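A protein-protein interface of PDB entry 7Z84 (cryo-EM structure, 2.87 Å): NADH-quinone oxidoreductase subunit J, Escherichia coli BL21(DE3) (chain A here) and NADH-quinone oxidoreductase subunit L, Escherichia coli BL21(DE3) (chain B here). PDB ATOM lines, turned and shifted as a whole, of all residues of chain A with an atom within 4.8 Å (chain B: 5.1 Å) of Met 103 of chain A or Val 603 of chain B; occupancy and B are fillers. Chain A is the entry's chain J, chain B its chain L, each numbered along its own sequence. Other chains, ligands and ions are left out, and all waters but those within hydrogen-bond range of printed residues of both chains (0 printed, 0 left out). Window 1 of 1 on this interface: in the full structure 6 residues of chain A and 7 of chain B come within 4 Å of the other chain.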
ATOM      1  N   LEU A  99      13.371  -1.672 -10.734  1.00  0.00           N
ATOM      2  CA  LEU A  99      14.762  -1.727 -10.290  1.00  0.00           C
ATOM      3  C   LEU A  99      15.307  -0.330 -10.019  1.00  0.00           C
ATOM      4  O   LEU A  99      15.857  -0.052  -8.942  1.00  0.00           O
ATOM      5  CB  LEU A  99      15.606  -2.426 -11.353  1.00  0.00           C
ATOM      6  CG  LEU A  99      16.745  -3.347 -10.935  1.00  0.00           C
ATOM      7  CD1 LEU A  99      16.247  -4.443 -10.017  1.00  0.00           C
ATOM      8  CD2 LEU A  99      17.380  -3.928 -12.182  1.00  0.00           C
ATOM      9  N   SER A 100      15.146   0.568 -10.994  1.00  0.00           N
ATOM     10  CA  SER A 100      15.556   1.954 -10.808  1.00  0.00           C
ATOM     11  C   SER A 100      14.741   2.631  -9.716  1.00  0.00           C
ATOM     12  O   SER A 100      15.251   3.518  -9.028  1.00  0.00           O
ATOM     13  CB  SER A 100      15.425   2.721 -12.120  1.00  0.00           C
ATOM     14  OG  SER A 100      16.569   2.537 -12.934  1.00  0.00           O
ATOM     15  N   ALA A 101      13.493   2.200  -9.518  1.00  0.00           N
ATOM     16  CA  ALA A 101      12.660   2.766  -8.466  1.00  0.00           C
ATOM     17  C   ALA A 101      13.200   2.428  -7.083  1.00  0.00           C
ATOM     18  O   ALA A 101      13.355   3.319  -6.242  1.00  0.00           O
ATOM     19  CB  ALA A 101      11.221   2.274  -8.618  1.00  0.00           C
ATOM     20  N   ILE A 102      13.497   1.148  -6.826  1.00  0.00           N
ATOM     21  CA  ILE A 102      13.999   0.789  -5.498  1.00  0.00           C
ATOM     22  C   ILE A 102      15.398   1.356  -5.283  1.00  0.00           C
ATOM     23  O   ILE A 102      15.743   1.755  -4.159  1.00  0.00           O
ATOM     24  CB  ILE A 102      13.958  -0.734  -5.255  1.00  0.00           C
ATOM     25  CG1 ILE A 102      14.681  -1.508  -6.357  1.00  0.00           C
ATOM     26  CG2 ILE A 102      12.516  -1.205  -5.112  1.00  0.00           C
ATOM     27  CD1 ILE A 102      14.479  -3.010  -6.299  1.00  0.00           C
ATOM     28  N   MET A 103      16.209   1.442  -6.347  1.00  0.00           N
ATOM     29  CA  MET A 103      17.497   2.121  -6.230  1.00  0.00           C
ATOM     30  C   MET A 103      17.313   3.596  -5.886  1.00  0.00           C
ATOM     31  O   MET A 103      18.058   4.149  -5.065  1.00  0.00           O
ATOM     32  CB  MET A 103      18.290   1.958  -7.526  1.00  0.00           C
ATOM     33  CG  MET A 103      19.581   2.754  -7.584  1.00  0.00           C
ATOM     34  SD  MET A 103      20.917   1.846  -8.381  1.00  0.00           S
ATOM     35  CE  MET A 103      20.026   1.023  -9.696  1.00  0.00           C
ATOM     36  N   LEU A 104      16.304   4.239  -6.479  1.00  0.00           N
ATOM     37  CA  LEU A 104      16.025   5.641  -6.191  1.00  0.00           C
ATOM     38  C   LEU A 104      15.564   5.839  -4.752  1.00  0.00           C
ATOM     39  O   LEU A 104      15.957   6.814  -4.109  1.00  0.00           O
ATOM     40  CB  LEU A 104      14.983   6.178  -7.171  1.00  0.00           C
ATOM     41  CG  LEU A 104      14.517   7.623  -6.989  1.00  0.00           C
ATOM     42  CD1 LEU A 104      15.691   8.584  -7.082  1.00  0.00           C
ATOM     43  CD2 LEU A 104      13.456   7.974  -8.017  1.00  0.00           C
ATOM     44  N   VAL A 105      14.731   4.932  -4.229  1.00  0.00           N
ATOM     45  CA  VAL A 105      14.301   5.060  -2.833  1.00  0.00           C
ATOM     46  C   VAL A 105      15.472   4.841  -1.878  1.00  0.00           C
ATOM     47  O   VAL A 105      15.574   5.518  -0.848  1.00  0.00           O
ATOM     48  CB  VAL A 105      13.120   4.125  -2.507  1.00  0.00           C
ATOM     49  CG1 VAL A 105      12.488   4.535  -1.191  1.00  0.00           C
ATOM     50  CG2 VAL A 105      12.049   4.244  -3.555  1.00  0.00           C
ATOM     51  N   VAL A 106      16.379   3.914  -2.201  1.00  0.00           N
ATOM     52  CA  VAL A 106      17.554   3.720  -1.349  1.00  0.00           C
ATOM     53  C   VAL A 106      18.455   4.957  -1.371  1.00  0.00           C
ATOM     54  O   VAL A 106      18.935   5.415  -0.321  1.00  0.00           O
ATOM     55  CB  VAL A 106      18.314   2.446  -1.764  1.00  0.00           C
ATOM     56  CG1 VAL A 106      19.650   2.365  -1.054  1.00  0.00           C
ATOM     57  CG2 VAL A 106      17.486   1.215  -1.443  1.00  0.00           C
ATOM     58  N   ILE A 107      18.673   5.536  -2.555  1.00  0.00           N
ATOM     59  CA  ILE A 107      19.506   6.733  -2.657  1.00  0.00           C
ATOM     60  C   ILE A 107      18.831   7.926  -1.978  1.00  0.00           C
ATOM     61  O   ILE A 107      19.497   8.765  -1.364  1.00  0.00           O
ATOM     62  CB  ILE A 107      19.854   7.011  -4.133  1.00  0.00           C
ATOM     63  CG1 ILE A 107      20.754   5.902  -4.677  1.00  0.00           C
ATOM     64  CG2 ILE A 107      20.604   8.312  -4.297  1.00  0.00           C
ATOM     65  CD1 ILE A 107      20.905   5.924  -6.179  1.00  0.00           C
ATOM     66  N   SER B 599      22.942  -3.117 -12.475  1.00  0.00           N
ATOM     67  CA  SER B 599      21.983  -2.368 -11.663  1.00  0.00           C
ATOM     68  C   SER B 599      21.426  -3.219 -10.525  1.00  0.00           C
ATOM     69  O   SER B 599      21.174  -2.706  -9.427  1.00  0.00           O
ATOM     70  CB  SER B 599      20.853  -1.832 -12.540  1.00  0.00           C
ATOM     71  OG  SER B 599      20.298  -2.858 -13.338  1.00  0.00           O
ATOM     72  N   ILE B 600      21.233  -4.521 -10.767  1.00  0.00           N
ATOM     73  CA  ILE B 600      20.804  -5.443  -9.715  1.00  0.00           C
ATOM     74  C   ILE B 600      21.850  -5.512  -8.612  1.00  0.00           C
ATOM     75  O   ILE B 600      21.521  -5.467  -7.418  1.00  0.00           O
ATOM     76  CB  ILE B 600      20.517  -6.834 -10.316  1.00  0.00           C
ATOM     77  CG1 ILE B 600      19.127  -6.879 -10.947  1.00  0.00           C
ATOM     78  CG2 ILE B 600      20.639  -7.937  -9.272  1.00  0.00           C
ATOM     79  CD1 ILE B 600      18.929  -8.038 -11.896  1.00  0.00           C
ATOM     80  N   GLY B 601      23.125  -5.608  -8.993  1.00  0.00           N
ATOM     81  CA  GLY B 601      24.188  -5.617  -8.006  1.00  0.00           C
ATOM     82  C   GLY B 601      24.295  -4.310  -7.247  1.00  0.00           C
ATOM     83  O   GLY B 601      24.591  -4.304  -6.052  1.00  0.00           O
ATOM     84  N   ALA B 602      24.046  -3.188  -7.929  1.00  0.00           N
ATOM     85  CA  ALA B 602      24.026  -1.896  -7.250  1.00  0.00           C
ATOM     86  C   ALA B 602      22.911  -1.828  -6.215  1.00  0.00           C
ATOM     87  O   ALA B 602      23.130  -1.370  -5.086  1.00  0.00           O
ATOM     88  CB  ALA B 602      23.881  -0.769  -8.271  1.00  0.00           C
ATOM     89  N   VAL B 603      21.717  -2.307  -6.579  1.00  0.00           N
ATOM     90  CA  VAL B 603      20.588  -2.326  -5.649  1.00  0.00           C
ATOM     91  C   VAL B 603      20.890  -3.229  -4.458  1.00  0.00           C
ATOM     92  O   VAL B 603      20.639  -2.860  -3.304  1.00  0.00           O
ATOM     93  CB  VAL B 603      19.305  -2.762  -6.382  1.00  0.00           C
ATOM     94  CG1 VAL B 603      18.192  -3.083  -5.394  1.00  0.00           C
ATOM     95  CG2 VAL B 603      18.854  -1.683  -7.346  1.00  0.00           C
ATOM     96  N   VAL B 604      21.457  -4.411  -4.718  1.00  0.00           N
ATOM     97  CA  VAL B 604      21.753  -5.367  -3.652  1.00  0.00           C
ATOM     98  C   VAL B 604      22.821  -4.818  -2.708  1.00  0.00           C
ATOM     99  O   VAL B 604      22.681  -4.902  -1.482  1.00  0.00           O
ATOM    100  CB  VAL B 604      22.161  -6.722  -4.261  1.00  0.00           C
ATOM    101  CG1 VAL B 604      22.855  -7.603  -3.233  1.00  0.00           C
ATOM    102  CG2 VAL B 604      20.944  -7.432  -4.825  1.00  0.00           C
ATOM    103  N   VAL B 605      23.885  -4.224  -3.261  1.00  0.00           N
ATOM    104  CA  VAL B 605      24.963  -3.674  -2.442  1.00  0.00           C
ATOM    105  C   VAL B 605      24.460  -2.506  -1.602  1.00  0.00           C
ATOM    106  O   VAL B 605      24.753  -2.417  -0.401  1.00  0.00           O
ATOM    107  CB  VAL B 605      26.151  -3.268  -3.341  1.00  0.00           C
ATOM    108  CG1 VAL B 605      27.052  -2.255  -2.649  1.00  0.00           C
ATOM    109  CG2 VAL B 605      26.948  -4.498  -3.746  1.00  0.00           C
ATOM    110  N   LEU B 606      23.672  -1.610  -2.206  1.00  0.00           N
ATOM    111  CA  LEU B 606      23.150  -0.464  -1.469  1.00  0.00           C
ATOM    112  C   LEU B 606      22.171  -0.892  -0.379  1.00  0.00           C
ATOM    113  O   LEU B 606      22.209  -0.360   0.737  1.00  0.00           O
ATOM    114  CB  LEU B 606      22.492   0.516  -2.438  1.00  0.00           C
ATOM    115  CG  LEU B 606      23.306   1.763  -2.784  1.00  0.00           C
ATOM    116  CD1 LEU B 606      24.545   1.396  -3.582  1.00  0.00           C
ATOM    117  CD2 LEU B 606      22.454   2.756  -3.552  1.00  0.00           C
ATOM    118  N   ALA B 607      21.305  -1.867  -0.673  1.00  0.00           N
ATOM    119  CA  ALA B 607      20.361  -2.351   0.329  1.00  0.00           C
ATOM    120  C   ALA B 607      21.075  -3.067   1.469  1.00  0.00           C
ATOM    121  O   ALA B 607      20.684  -2.928   2.634  1.00  0.00           O
ATOM    122  CB  ALA B 607      19.332  -3.274  -0.325  1.00  0.00           C
ATOM    123  N   LEU B 608      22.121  -3.837   1.153  1.00  0.00           N
ATOM    124  CA  LEU B 608      22.890  -4.507   2.196  1.00  0.00           C
ATOM    125  C   LEU B 608      23.644  -3.503   3.058  1.00  0.00           C
ATOM    126  O   LEU B 608      23.779  -3.697   4.271  1.00  0.00           O
ATOM    127  CB  LEU B 608      23.858  -5.511   1.570  1.00  0.00           C
ATOM    128  CG  LEU B 608      23.474  -6.995   1.573  1.00  0.00           C
ATOM    129  CD1 LEU B 608      23.874  -7.647   2.886  1.00  0.00           C
ATOM    130  CD2 LEU B 608      21.991  -7.200   1.299  1.00  0.00           C
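Printed residues of chain A that touch a printed residue of chain B: Leu 99, Ile 102, Met 103, Val 106 and Ile 107. Hydrophobic or aromatic side chains of chain A within 4 Å of the printed part of chain B: Leu 99, Ile 102, Met 103, Val 106 and Ile 107. Of the 10 printed residues of chain B, 5 touch a printed residue of chain A. Among the printed residues, no Asp or Glu carboxylate lies within 4 Å of a Lys or Arg side-chain nitrogen of the other chain.
Printed residues of chain B within 4 Å of Ile 102 of chain A: Val 603. Met 103 of chain A touches just these residues of chain B: Ser 599, Ala 602 and Val 603. Of the printed residues of chain A, Ser 599 of chain B touches Leu 99 and Met 103. Val 603 of chain B touches just these residues of chain A: Leu 99 (3.8 Å), Ile 102 (3.8 Å) and Met 103 (3.7 Å). Val 605 of chain B touches none of the printed residues of chain A. Printed residues of chain A within 4 Å of Leu 606 of chain B: Val 106 and Ile 107. The nearest residue of chain B that does not touch Met 103 of chain A is Leu 606 of chain B (4.9 Å). The nearest printed residue of chain A that does not touch Val 603 of chain B is Val 106 of chain A (5.5 Å).
Among the printed residues, merely in contact across the chains: Leu 99 of chain A with Ser 599 of chain B (3.3 Å), Leu 99 of chain A with Ile 600 of chain B (3.6 Å), Leu 99 of chain A with Val 603 of chain B (3.8 Å), Ile 102 of chain A with Val 603 of chain B (3.8 Å), Met 103 of chain A with Ser 599 of chain B (3.9 Å), Met 103 of chain A with Ala 602 of chain B (3.95 Å), Met 103 of chain A with Val 603 of chain B (3.7 Å), Val 106 of chain A with Leu 606 of chain B (3.7 Å) and Ile 107 of chain A with Leu 606 of chain B (3.7 Å).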
